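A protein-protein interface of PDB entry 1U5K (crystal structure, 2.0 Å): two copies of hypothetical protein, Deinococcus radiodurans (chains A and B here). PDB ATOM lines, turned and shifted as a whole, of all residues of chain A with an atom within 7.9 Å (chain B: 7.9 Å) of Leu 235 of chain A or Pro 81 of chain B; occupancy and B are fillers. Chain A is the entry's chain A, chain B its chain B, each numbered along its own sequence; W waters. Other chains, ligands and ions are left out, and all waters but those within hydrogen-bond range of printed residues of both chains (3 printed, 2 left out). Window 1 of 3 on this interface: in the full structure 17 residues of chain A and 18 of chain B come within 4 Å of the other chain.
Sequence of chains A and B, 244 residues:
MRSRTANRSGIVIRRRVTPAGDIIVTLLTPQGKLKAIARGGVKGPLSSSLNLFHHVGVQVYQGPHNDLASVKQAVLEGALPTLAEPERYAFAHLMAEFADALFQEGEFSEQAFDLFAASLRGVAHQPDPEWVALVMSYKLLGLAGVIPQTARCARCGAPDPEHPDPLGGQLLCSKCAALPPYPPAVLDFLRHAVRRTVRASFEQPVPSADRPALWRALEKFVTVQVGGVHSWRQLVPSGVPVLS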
ATOM      1  N   PHE A  53     -24.063  20.761  21.225  1.00  0.00           N
ATOM      2  CA  PHE A  53     -24.152  19.392  21.695  1.00  0.00           C
ATOM      3  C   PHE A  53     -25.433  19.109  22.480  1.00  0.00           C
ATOM      4  O   PHE A  53     -25.690  17.970  22.846  1.00  0.00           O
ATOM      5  CB  PHE A  53     -22.887  18.935  22.432  1.00  0.00           C
ATOM      6  CG  PHE A  53     -21.594  19.367  21.773  1.00  0.00           C
ATOM      7  CD1 PHE A  53     -20.589  19.971  22.510  1.00  0.00           C
ATOM      8  CD2 PHE A  53     -21.418  19.278  20.407  1.00  0.00           C
ATOM      9  CE1 PHE A  53     -19.398  20.404  21.918  1.00  0.00           C
ATOM     10  CE2 PHE A  53     -20.253  19.712  19.809  1.00  0.00           C
ATOM     11  CZ  PHE A  53     -19.236  20.279  20.548  1.00  0.00           C
ATOM     12  N   TYR A  89     -14.897  17.795  24.899  1.00  0.00           N
ATOM     13  CA  TYR A  89     -15.408  18.862  24.060  1.00  0.00           C
ATOM     14  C   TYR A  89     -14.761  18.829  22.677  1.00  0.00           C
ATOM     15  O   TYR A  89     -15.463  18.917  21.676  1.00  0.00           O
ATOM     16  CB  TYR A  89     -15.204  20.227  24.717  1.00  0.00           C
ATOM     17  CG  TYR A  89     -15.900  21.357  24.019  1.00  0.00           C
ATOM     18  CD1 TYR A  89     -17.096  21.865  24.508  1.00  0.00           C
ATOM     19  CD2 TYR A  89     -15.332  21.972  22.898  1.00  0.00           C
ATOM     20  CE1 TYR A  89     -17.724  22.925  23.885  1.00  0.00           C
ATOM     21  CE2 TYR A  89     -15.948  23.042  22.271  1.00  0.00           C
ATOM     22  CZ  TYR A  89     -17.143  23.519  22.789  1.00  0.00           C
ATOM     23  OH  TYR A  89     -17.810  24.571  22.195  1.00  0.00           O
ATOM     24  N   ALA A  90     -13.446  18.667  22.636  1.00  0.00           N
ATOM     25  CA  ALA A  90     -12.669  18.690  21.406  1.00  0.00           C
ATOM     26  C   ALA A  90     -13.116  17.604  20.439  1.00  0.00           C
ATOM     27  O   ALA A  90     -13.223  17.869  19.250  1.00  0.00           O
ATOM     28  CB  ALA A  90     -11.165  18.595  21.696  1.00  0.00           C
ATOM     29  N   PHE A  91     -13.382  16.401  20.940  1.00  0.00           N
ATOM     30  CA  PHE A  91     -13.834  15.291  20.116  1.00  0.00           C
ATOM     31  C   PHE A  91     -15.305  15.418  19.712  1.00  0.00           C
ATOM     32  O   PHE A  91     -15.622  15.086  18.571  1.00  0.00           O
ATOM     33  CB  PHE A  91     -13.458  13.938  20.735  1.00  0.00           C
ATOM     34  CG  PHE A  91     -11.993  13.617  20.606  1.00  0.00           C
ATOM     35  CD1 PHE A  91     -11.170  13.561  21.721  1.00  0.00           C
ATOM     36  CD2 PHE A  91     -11.415  13.427  19.352  1.00  0.00           C
ATOM     37  CE1 PHE A  91      -9.792  13.349  21.586  1.00  0.00           C
ATOM     38  CE2 PHE A  91     -10.058  13.170  19.224  1.00  0.00           C
ATOM     39  CZ  PHE A  91      -9.224  13.145  20.341  1.00  0.00           C
ATOM     40  N   ALA A  92     -16.180  15.914  20.589  1.00  0.00           N
ATOM     41  CA  ALA A  92     -17.557  16.240  20.236  1.00  0.00           C
ATOM     42  C   ALA A  92     -17.557  17.237  19.078  1.00  0.00           C
ATOM     43  O   ALA A  92     -18.317  17.102  18.125  1.00  0.00           O
ATOM     44  CB  ALA A  92     -18.356  16.813  21.435  1.00  0.00           C
ATOM     45  N   HIS A  93     -16.701  18.246  19.176  1.00  0.00           N
ATOM     46  CA  HIS A  93     -16.604  19.312  18.188  1.00  0.00           C
ATOM     47  C   HIS A  93     -16.119  18.787  16.833  1.00  0.00           C
ATOM     48  O   HIS A  93     -16.667  19.147  15.798  1.00  0.00           O
ATOM     49  CB  HIS A  93     -15.665  20.345  18.766  1.00  0.00           C
ATOM     50  CG  HIS A  93     -15.653  21.676  18.085  1.00  0.00           C
ATOM     51  ND1 HIS A  93     -16.730  22.185  17.395  1.00  0.00           N
ATOM     52  CD2 HIS A  93     -14.700  22.637  18.058  1.00  0.00           C
ATOM     53  CE1 HIS A  93     -16.434  23.393  16.953  1.00  0.00           C
ATOM     54  NE2 HIS A  93     -15.197  23.677  17.314  1.00  0.00           N
ATOM     55  N   LEU A  94     -15.127  17.907  16.851  1.00  0.00           N
ATOM     56  CA  LEU A  94     -14.703  17.199  15.656  1.00  0.00           C
ATOM     57  C   LEU A  94     -15.855  16.421  15.014  1.00  0.00           C
ATOM     58  O   LEU A  94     -16.065  16.540  13.811  1.00  0.00           O
ATOM     59  CB  LEU A  94     -13.501  16.309  15.950  1.00  0.00           C
ATOM     60  CG  LEU A  94     -13.003  15.352  14.872  1.00  0.00           C
ATOM     61  CD1 LEU A  94     -12.669  16.099  13.599  1.00  0.00           C
ATOM     62  CD2 LEU A  94     -11.783  14.634  15.404  1.00  0.00           C
ATOM     63  N   MET A  95     -16.596  15.627  15.779  1.00  0.00           N
ATOM     64  CA  MET A  95     -17.682  14.834  15.194  1.00  0.00           C
ATOM     65  C   MET A  95     -18.689  15.774  14.546  1.00  0.00           C
ATOM     66  O   MET A  95     -19.179  15.455  13.469  1.00  0.00           O
ATOM     67  CB  MET A  95     -18.403  13.976  16.227  1.00  0.00           C
ATOM     68  CG  MET A  95     -17.468  12.928  16.811  1.00  0.00           C
ATOM     69  SD  MET A  95     -16.846  11.732  15.641  1.00  0.00           S
ATOM     70  CE  MET A  95     -15.443  12.504  15.017  1.00  0.00           C
ATOM     71  N   ALA A  96     -18.989  16.890  15.204  1.00  0.00           N
ATOM     72  CA  ALA A  96     -19.982  17.830  14.709  1.00  0.00           C
ATOM     73  C   ALA A  96     -19.600  18.404  13.340  1.00  0.00           C
ATOM     74  O   ALA A  96     -20.389  18.340  12.394  1.00  0.00           O
ATOM     75  CB  ALA A  96     -20.251  18.917  15.711  1.00  0.00           C
ATOM     76  N   GLU A  97     -18.386  18.938  13.238  1.00  0.00           N
ATOM     77  CA  GLU A  97     -17.931  19.578  12.003  1.00  0.00           C
ATOM     78  C   GLU A  97     -17.657  18.521  10.925  1.00  0.00           C
ATOM     79  O   GLU A  97     -17.933  18.710   9.745  1.00  0.00           O
ATOM     80  CB  GLU A  97     -16.725  20.485  12.279  1.00  0.00           C
ATOM     81  CG  GLU A  97     -17.058  21.724  13.103  1.00  0.00           C
ATOM     82  CD  GLU A  97     -17.868  22.766  12.338  1.00  0.00           C
ATOM     83  OE1 GLU A  97     -18.060  22.658  11.102  1.00  0.00           O
ATOM     84  OE2 GLU A  97     -18.306  23.739  12.980  1.00  0.00           O
ATOM     85  N   PHE A  98     -17.205  17.340  11.338  1.00  0.00           N
ATOM     86  CA  PHE A  98     -16.940  16.267  10.396  1.00  0.00           C
ATOM     87  C   PHE A  98     -18.251  15.794   9.783  1.00  0.00           C
ATOM     88  O   PHE A  98     -18.359  15.662   8.559  1.00  0.00           O
ATOM     89  CB  PHE A  98     -16.248  15.084  11.082  1.00  0.00           C
ATOM     90  CG  PHE A  98     -16.131  13.867  10.213  1.00  0.00           C
ATOM     91  CD1 PHE A  98     -15.154  13.767   9.234  1.00  0.00           C
ATOM     92  CD2 PHE A  98     -17.015  12.814  10.377  1.00  0.00           C
ATOM     93  CE1 PHE A  98     -15.061  12.611   8.434  1.00  0.00           C
ATOM     94  CE2 PHE A  98     -16.909  11.668   9.604  1.00  0.00           C
ATOM     95  CZ  PHE A  98     -15.951  11.582   8.616  1.00  0.00           C
ATOM     96  N   TRP A 215      -6.069   8.857  11.057  1.00  0.00           N
ATOM     97  CA  TRP A 215      -6.597  10.197  10.866  1.00  0.00           C
ATOM     98  C   TRP A 215      -6.215  10.699   9.486  1.00  0.00           C
ATOM     99  O   TRP A 215      -7.030  11.323   8.812  1.00  0.00           O
ATOM    100  CB  TRP A 215      -6.113  11.199  11.914  1.00  0.00           C
ATOM    101  CG  TRP A 215      -6.801  11.041  13.219  1.00  0.00           C
ATOM    102  CD1 TRP A 215      -6.205  10.683  14.399  1.00  0.00           C
ATOM    103  CD2 TRP A 215      -8.200  11.185  13.494  1.00  0.00           C
ATOM    104  NE1 TRP A 215      -7.149  10.612  15.388  1.00  0.00           N
ATOM    105  CE2 TRP A 215      -8.379  10.923  14.868  1.00  0.00           C
ATOM    106  CE3 TRP A 215      -9.327  11.493  12.727  1.00  0.00           C
ATOM    107  CZ2 TRP A 215      -9.628  10.953  15.478  1.00  0.00           C
ATOM    108  CZ3 TRP A 215     -10.575  11.530  13.342  1.00  0.00           C
ATOM    109  CH2 TRP A 215     -10.719  11.232  14.703  1.00  0.00           C
ATOM    110  N   GLU A 219      -8.715  11.869   6.350  1.00  0.00           N
ATOM    111  CA  GLU A 219      -8.651  13.229   5.831  1.00  0.00           C
ATOM    112  C   GLU A 219      -8.476  13.257   4.313  1.00  0.00           C
ATOM    113  O   GLU A 219      -9.178  13.999   3.636  1.00  0.00           O
ATOM    114  CB  GLU A 219      -7.498  14.003   6.473  1.00  0.00           C
ATOM    115  CG  GLU A 219      -7.732  14.393   7.919  1.00  0.00           C
ATOM    116  CD  GLU A 219      -6.576  15.192   8.505  1.00  0.00           C
ATOM    117  OE1 GLU A 219      -6.661  16.428   8.514  1.00  0.00           O
ATOM    118  OE2 GLU A 219      -5.556  14.616   8.924  1.00  0.00           O
ATOM    119  N   HIS A 230     -13.519  21.458   4.090  1.00  0.00           N
ATOM    120  CA  HIS A 230     -13.033  20.498   5.078  1.00  0.00           C
ATOM    121  C   HIS A 230     -12.221  21.182   6.185  1.00  0.00           C
ATOM    122  O   HIS A 230     -11.134  20.759   6.588  1.00  0.00           O
ATOM    123  CB  HIS A 230     -12.322  19.343   4.363  1.00  0.00           C
ATOM    124  CG  HIS A 230     -13.245  18.569   3.470  1.00  0.00           C
ATOM    125  ND1 HIS A 230     -14.321  17.865   3.957  1.00  0.00           N
ATOM    126  CD2 HIS A 230     -13.332  18.500   2.121  1.00  0.00           C
ATOM    127  CE1 HIS A 230     -15.022  17.378   2.952  1.00  0.00           C
ATOM    128  NE2 HIS A 230     -14.431  17.735   1.827  1.00  0.00           N
ATOM    129  N   SER A 231     -12.826  22.242   6.710  1.00  0.00           N
ATOM    130  CA  SER A 231     -12.358  22.935   7.906  1.00  0.00           C
ATOM    131  C   SER A 231     -12.366  22.079   9.175  1.00  0.00           C
ATOM    132  O   SER A 231     -11.746  22.374  10.194  1.00  0.00           O
ATOM    133  CB  SER A 231     -13.155  24.229   8.073  1.00  0.00           C
ATOM    134  OG  SER A 231     -14.546  24.013   8.230  1.00  0.00           O
ATOM    135  N   TRP A 232     -13.136  21.007   9.168  1.00  0.00           N
ATOM    136  CA  TRP A 232     -13.142  20.072  10.280  1.00  0.00           C
ATOM    137  C   TRP A 232     -11.770  19.489  10.551  1.00  0.00           C
ATOM    138  O   TRP A 232     -11.497  19.017  11.650  1.00  0.00           O
ATOM    139  CB  TRP A 232     -14.144  18.951  10.009  1.00  0.00           C
ATOM    140  CG  TRP A 232     -13.813  18.078   8.854  1.00  0.00           C
ATOM    141  CD1 TRP A 232     -14.249  18.236   7.581  1.00  0.00           C
ATOM    142  CD2 TRP A 232     -12.991  16.904   8.864  1.00  0.00           C
ATOM    143  NE1 TRP A 232     -13.718  17.258   6.780  1.00  0.00           N
ATOM    144  CE2 TRP A 232     -12.954  16.415   7.546  1.00  0.00           C
ATOM    145  CE3 TRP A 232     -12.283  16.211   9.846  1.00  0.00           C
ATOM    146  CZ2 TRP A 232     -12.258  15.254   7.195  1.00  0.00           C
ATOM    147  CZ3 TRP A 232     -11.576  15.058   9.493  1.00  0.00           C
ATOM    148  CH2 TRP A 232     -11.550  14.608   8.172  1.00  0.00           C
ATOM    149  N   ARG A 233     -10.877  19.538   9.567  1.00  0.00           N
ATOM    150  CA  ARG A 233      -9.507  19.090   9.774  1.00  0.00           C
ATOM    151  C   ARG A 233      -8.680  19.913  10.764  1.00  0.00           C
ATOM    152  O   ARG A 233      -7.729  19.388  11.320  1.00  0.00           O
ATOM    153  CB  ARG A 233      -8.764  19.015   8.451  1.00  0.00           C
ATOM    154  CG  ARG A 233      -9.296  17.915   7.570  1.00  0.00           C
ATOM    155  CD  ARG A 233      -9.518  18.361   6.170  1.00  0.00           C
ATOM    156  NE  ARG A 233      -8.289  18.586   5.459  1.00  0.00           N
ATOM    157  CZ  ARG A 233      -8.026  19.620   4.664  1.00  0.00           C
ATOM    158  NH1 ARG A 233      -8.846  20.646   4.469  1.00  0.00           N
ATOM    159  NH2 ARG A 233      -6.852  19.633   4.051  1.00  0.00           N
ATOM    160  N   GLN A 234      -9.121  21.127  11.071  1.00  0.00           N
ATOM    161  CA  GLN A 234      -8.601  21.906  12.190  1.00  0.00           C
ATOM    162  C   GLN A 234      -8.714  21.185  13.540  1.00  0.00           C
ATOM    163  O   GLN A 234      -7.954  21.433  14.484  1.00  0.00           O
ATOM    164  CB  GLN A 234      -9.377  23.217  12.245  1.00  0.00           C
ATOM    165  CG  GLN A 234      -9.142  24.149  11.081  1.00  0.00           C
ATOM    166  CD  GLN A 234      -7.656  24.440  10.928  1.00  0.00           C
ATOM    167  OE1 GLN A 234      -7.028  25.026  11.817  1.00  0.00           O
ATOM    168  NE2 GLN A 234      -7.078  23.960   9.845  1.00  0.00           N
ATOM    169  N   LEU A 235      -9.678  20.277  13.647  1.00  0.00           N
ATOM    170  CA  LEU A 235      -9.916  19.581  14.896  1.00  0.00           C
ATOM    171  C   LEU A 235      -9.340  18.171  15.019  1.00  0.00           C
ATOM    172  O   LEU A 235      -9.492  17.535  16.063  1.00  0.00           O
ATOM    173  CB  LEU A 235     -11.418  19.559  15.175  1.00  0.00           C
ATOM    174  CG  LEU A 235     -12.071  20.933  15.159  1.00  0.00           C
ATOM    175  CD1 LEU A 235     -13.573  20.798  15.294  1.00  0.00           C
ATOM    176  CD2 LEU A 235     -11.483  21.907  16.176  1.00  0.00           C
ATOM    177  N   VAL A 236      -8.676  17.674  13.979  1.00  0.00           N
ATOM    178  CA  VAL A 236      -8.070  16.345  14.061  1.00  0.00           C
ATOM    179  C   VAL A 236      -6.883  16.419  15.022  1.00  0.00           C
ATOM    180  O   VAL A 236      -6.187  17.427  14.997  1.00  0.00           O
ATOM    181  CB  VAL A 236      -7.660  15.886  12.652  1.00  0.00           C
ATOM    182  CG1 VAL A 236      -6.869  14.590  12.693  1.00  0.00           C
ATOM    183  CG2 VAL A 236      -8.896  15.689  11.800  1.00  0.00           C
ATOM    184  N   PRO A 237      -6.669  15.462  15.924  1.00  0.00           N
ATOM    185  CA  PRO A 237      -5.568  15.575  16.892  1.00  0.00           C
ATOM    186  C   PRO A 237      -4.251  15.934  16.207  1.00  0.00           C
ATOM    187  O   PRO A 237      -3.905  15.303  15.210  1.00  0.00           O
ATOM    188  CB  PRO A 237      -5.452  14.169  17.488  1.00  0.00           C
ATOM    189  CG  PRO A 237      -6.817  13.588  17.352  1.00  0.00           C
ATOM    190  CD  PRO A 237      -7.427  14.216  16.122  1.00  0.00           C
ATOM    191  N   SER A 238      -3.580  16.958  16.723  1.00  0.00           N
ATOM    192  CA  SER A 238      -2.414  17.574  16.095  1.00  0.00           C
ATOM    193  C   SER A 238      -1.383  18.125  17.086  1.00  0.00           C
ATOM    194  O   SER A 238      -0.540  18.947  16.711  1.00  0.00           O
ATOM    195  CB  SER A 238      -2.902  18.716  15.201  1.00  0.00           C
ATOM    196  OG  SER A 238      -3.931  18.242  14.343  1.00  0.00           O
ATOM    197  N   ASN B  51      -0.479  22.186  12.202  1.00  0.00           N
ATOM    198  CA  ASN B  51      -1.750  22.424  11.524  1.00  0.00           C
ATOM    199  C   ASN B  51      -1.942  23.899  11.178  1.00  0.00           C
ATOM    200  O   ASN B  51      -1.423  24.809  11.830  1.00  0.00           O
ATOM    201  CB  ASN B  51      -2.905  21.882  12.375  1.00  0.00           C
ATOM    202  CG  ASN B  51      -4.035  21.258  11.554  1.00  0.00           C
ATOM    203  OD1 ASN B  51      -4.898  20.547  12.094  1.00  0.00           O
ATOM    204  ND2 ASN B  51      -4.056  21.547  10.261  1.00  0.00           N
ATOM    205  N   HIS B  54      -2.387  27.219  13.412  1.00  0.00           N
ATOM    206  CA  HIS B  54      -1.851  26.999  14.745  1.00  0.00           C
ATOM    207  C   HIS B  54      -0.650  27.888  15.048  1.00  0.00           C
ATOM    208  O   HIS B  54       0.148  28.222  14.172  1.00  0.00           O
ATOM    209  CB  HIS B  54      -1.486  25.532  14.985  1.00  0.00           C
ATOM    210  CG  HIS B  54      -2.666  24.623  15.142  1.00  0.00           C
ATOM    211  ND1 HIS B  54      -2.529  23.303  15.513  1.00  0.00           N
ATOM    212  CD2 HIS B  54      -3.994  24.838  14.993  1.00  0.00           C
ATOM    213  CE1 HIS B  54      -3.728  22.758  15.623  1.00  0.00           C
ATOM    214  NE2 HIS B  54      -4.635  23.662  15.300  1.00  0.00           N
ATOM    215  N   GLY B  78      -0.738  27.321  20.795  1.00  0.00           N
ATOM    216  CA  GLY B  78      -2.162  27.564  20.944  1.00  0.00           C
ATOM    217  C   GLY B  78      -2.898  27.425  19.626  1.00  0.00           C
ATOM    218  O   GLY B  78      -2.303  27.456  18.545  1.00  0.00           O
ATOM    219  N   ALA B  79      -4.205  27.237  19.741  1.00  0.00           N
ATOM    220  CA  ALA B  79      -5.065  27.006  18.594  1.00  0.00           C
ATOM    221  C   ALA B  79      -6.402  27.695  18.812  1.00  0.00           C
ATOM    222  O   ALA B  79      -6.775  27.999  19.949  1.00  0.00           O
ATOM    223  CB  ALA B  79      -5.259  25.526  18.399  1.00  0.00           C
ATOM    224  N   LEU B  80      -7.077  27.985  17.706  1.00  0.00           N
ATOM    225  CA  LEU B  80      -8.393  28.610  17.706  1.00  0.00           C
ATOM    226  C   LEU B  80      -9.399  27.603  17.148  1.00  0.00           C
ATOM    227  O   LEU B  80      -9.550  27.511  15.931  1.00  0.00           O
ATOM    228  CB  LEU B  80      -8.329  29.878  16.861  1.00  0.00           C
ATOM    229  CG  LEU B  80      -7.488  31.016  17.432  1.00  0.00           C
ATOM    230  CD1 LEU B  80      -7.176  32.019  16.370  1.00  0.00           C
ATOM    231  CD2 LEU B  80      -8.103  31.628  18.694  1.00  0.00           C
ATOM    232  N   PRO B  81      -9.999  26.774  17.994  1.00  0.00           N
ATOM    233  CA  PRO B  81     -10.867  25.700  17.489  1.00  0.00           C
ATOM    234  C   PRO B  81     -12.040  26.174  16.635  1.00  0.00           C
ATOM    235  O   PRO B  81     -12.461  25.418  15.762  1.00  0.00           O
ATOM    236  CB  PRO B  81     -11.377  24.985  18.748  1.00  0.00           C
ATOM    237  CG  PRO B  81     -10.947  25.806  19.913  1.00  0.00           C
ATOM    238  CD  PRO B  81      -9.821  26.719  19.456  1.00  0.00           C
ATOM    239  N   THR B  82     -12.562  27.380  16.854  1.00  0.00           N
ATOM    240  CA  THR B  82     -13.716  27.827  16.074  1.00  0.00           C
ATOM    241  C   THR B  82     -13.377  28.184  14.639  1.00  0.00           C
ATOM    242  O   THR B  82     -14.278  28.412  13.824  1.00  0.00           O
ATOM    243  CB  THR B  82     -14.404  29.041  16.711  1.00  0.00           C
ATOM    244  OG1 THR B  82     -13.480  30.133  16.730  1.00  0.00           O
ATOM    245  CG2 THR B  82     -14.765  28.782  18.187  1.00  0.00           C
ATOM    246  N   LEU B  83     -12.088  28.207  14.316  1.00  0.00           N
ATOM    247  CA  LEU B  83     -11.674  28.244  12.917  1.00  0.00           C
ATOM    248  C   LEU B  83     -12.069  26.977  12.148  1.00  0.00           C
ATOM    249  O   LEU B  83     -11.920  26.905  10.933  1.00  0.00           O
ATOM    250  CB  LEU B  83     -10.171  28.510  12.799  1.00  0.00           C
ATOM    251  CG  LEU B  83      -9.731  29.909  13.240  1.00  0.00           C
ATOM    252  CD1 LEU B  83      -8.265  30.132  12.979  1.00  0.00           C
ATOM    253  CD2 LEU B  83     -10.564  31.049  12.638  1.00  0.00           C
ATOM    254  N   ALA B  84     -12.598  25.982  12.850  1.00  0.00           N
ATOM    255  CA  ALA B  84     -13.129  24.782  12.226  1.00  0.00           C
ATOM    256  C   ALA B  84     -14.482  25.022  11.563  1.00  0.00           C
ATOM    257  O   ALA B  84     -14.943  24.192  10.781  1.00  0.00           O
ATOM    258  CB  ALA B  84     -13.244  23.694  13.255  1.00  0.00           C
ATOM    259  N   GLU B  85     -15.110  26.151  11.887  1.00  0.00           N
ATOM    260  CA  GLU B  85     -16.397  26.518  11.320  1.00  0.00           C
ATOM    261  C   GLU B  85     -16.112  27.028   9.919  1.00  0.00           C
ATOM    262  O   GLU B  85     -15.243  27.889   9.769  1.00  0.00           O
ATOM    263  CB  GLU B  85     -17.090  27.594  12.156  1.00  0.00           C
ATOM    264  CG  GLU B  85     -17.294  27.237  13.620  1.00  0.00           C
ATOM    265  CD  GLU B  85     -17.969  28.334  14.424  1.00  0.00           C
ATOM    266  OE1 GLU B  85     -18.428  29.341  13.833  1.00  0.00           O
ATOM    267  OE2 GLU B  85     -18.077  28.137  15.649  1.00  0.00           O
ATOM    268  N   ARG B  88     -15.687  30.828   9.189  1.00  0.00           N
ATOM    269  CA  ARG B  88     -14.546  31.406   9.877  1.00  0.00           C
ATOM    270  C   ARG B  88     -13.237  30.903   9.264  1.00  0.00           C
ATOM    271  O   ARG B  88     -12.284  31.672   9.101  1.00  0.00           O
ATOM    272  CB  ARG B  88     -14.646  31.132  11.372  1.00  0.00           C
ATOM    273  CG  ARG B  88     -15.838  31.760  12.060  1.00  0.00           C
ATOM    274  CD  ARG B  88     -15.796  31.455  13.540  1.00  0.00           C
ATOM    275  NE  ARG B  88     -17.006  31.862  14.245  1.00  0.00           N
ATOM    276  CZ  ARG B  88     -17.316  33.096  14.599  1.00  0.00           C
ATOM    277  NH1 ARG B  88     -18.451  33.283  15.251  1.00  0.00           N
ATOM    278  NH2 ARG B  88     -16.536  34.125  14.288  1.00  0.00           N
ATOM    279  N   ALA B 124     -12.008  34.260  14.493  1.00  0.00           N
ATOM    280  CA  ALA B 124     -12.420  33.138  15.333  1.00  0.00           C
ATOM    281  C   ALA B 124     -13.569  33.454  16.274  1.00  0.00           C
ATOM    282  O   ALA B 124     -14.449  32.607  16.464  1.00  0.00           O
ATOM    283  CB  ALA B 124     -11.271  32.640  16.149  1.00  0.00           C
ATOM    284  N   HIS B 125     -13.575  34.658  16.835  1.00  0.00           N
ATOM    285  CA  HIS B 125     -14.394  34.950  18.002  1.00  0.00           C
ATOM    286  C   HIS B 125     -15.544  35.933  17.830  1.00  0.00           C
ATOM    287  O   HIS B 125     -16.529  35.854  18.546  1.00  0.00           O
ATOM    288  CB  HIS B 125     -13.547  35.500  19.130  1.00  0.00           C
ATOM    289  CG  HIS B 125     -12.472  34.579  19.593  1.00  0.00           C
ATOM    290  ND1 HIS B 125     -12.717  33.290  20.001  1.00  0.00           N
ATOM    291  CD2 HIS B 125     -11.145  34.789  19.759  1.00  0.00           C
ATOM    292  CE1 HIS B 125     -11.579  32.733  20.372  1.00  0.00           C
ATOM    293  NE2 HIS B 125     -10.617  33.631  20.264  1.00  0.00           N
HETATM  294  O   HOH W   1      -7.507  23.710  15.862  1.00  0.00           O
HETATM  295  O   HOH W   2      -7.877  26.004  14.435  1.00  0.00           O
HETATM  296  O   HOH W   3      -0.321  21.523  15.453  1.00  0.00           O
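The backbone carbonyl oxygen (O) of Ala 84 of chain B lies within hydrogen-bond range of the side-chain hydroxyl (OG) of Ser 231 of chain A (2.6 Å). O of Arg 233 of chain A sits close to OD1 of Asn 51 of chain B (3.2 Å). OG of Ser 238 of chain A lies within hydrogen-bond range of OD1 of Asn 51 of chain B (3.4 Å). OE1 of Glu 97 of chain A lies close to O of Ala 84 of chain B, 3.5 Å away.
The backbone carbonyl oxygen of His 230 of chain A lies close to the guanidinium group of Arg 233 of chain A (3.1 Å). The backbone carbonyl oxygen (O) of Val 236 of chain A sits at hydrogen-bond distance from the side-chain hydroxyl (OG) of Ser 238 of chain A, 2.5 Å away. The guanidinium group (NE) of Arg 88 of chain B is in salt-bridge range of the side-chain carboxylate (OE1) of Glu 85 of chain B (2.9 Å).
Among the printed residues, merely in contact across the chains: His 93 of chain A with Pro 81 of chain B (3.6 Å), Glu 97 of chain A with Glu 85 of chain B (3.7 Å), Ser 231 of chain A with Glu 85 of chain B (3.8 Å), Gln 234 of chain A with Asn 51 of chain B (3.9 Å), Gln 234 of chain A with Leu 83 of chain B (3.9 Å), Leu 235 of chain A with Pro 81 of chain B (3.7 Å) and Leu 235 of chain A with Ala 84 of chain B (3.6 Å).
Of chain B, only Pro 81 (3.7 Å) and Ala 84 (3.6 Å) come within 4 Å of Leu 235 of chain A. Of chain A, only His 93 (3.6 Å) and Leu 235 (3.7 Å) come within 4 Å of Pro 81 of chain B. Of the printed residues of chain A, Leu 83 of chain B touches Gln 234. Of the printed residues of chain A, Asn 51 of chain B touches Arg 233 (3.2 Å), Gln 234 (3.9 Å) and Ser 238 (3.4 Å). Of the printed residues of chain B, His 93 of chain A touches Pro 81 (3.6 Å). Printed residues of chain B within 4 Å of Arg 233 of chain A: Asn 51. Printed residues of chain B within 4 Å of Glu 97 of chain A: Ala 84 and Glu 85. Arg 88 of chain B touches none of the printed residues of chain A. Trp 215 of chain A touches none of the printed residues of chain B. The nearest residue of chain B that does not touch Leu 235 of chain A is Asn 51 of chain B (5.0 Å). The nearest residue of chain A that does not touch Pro 81 of chain B is Gln 234 of chain A (5.2 Å). The nearest printed residue of chain B that does not touch Ser 231 of chain A is Leu 83 of chain B (4.1 Å).
Of the 22 printed residues of chain A, 7 touch a printed residue of chain B. Printed residues of chain A that touch a printed residue of chain B: His 93, Glu 97, Ser 231, Arg 233, Gln 234, Leu 235 and Ser 238. Hydrophobic or aromatic side chains of chain A within 4 Å of the printed part of chain B: His 93 and Leu 235. Hydrophobic or aromatic side chains of chain B within 4 Å of the printed part of chain A: Ala 84.
No position is printed for both chains.
Water W1 bridges O of Gln 234 of chain A (2.7 Å) and NE2 of His 54 of chain B (2.9 Å). Water W2 lies within hydrogen-bond range of O of Leu 80 of chain B and OE1 of Gln 234 of chain A. Water W3 lies within hydrogen-bond range of a ring nitrogen (ND1) of His 54 of chain B (2.8 Å), the backbone carbonyl oxygen of Ser 238 of chain A (2.9 Å) and the backbone NH of Asn 51 of chain B (3.3 Å).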
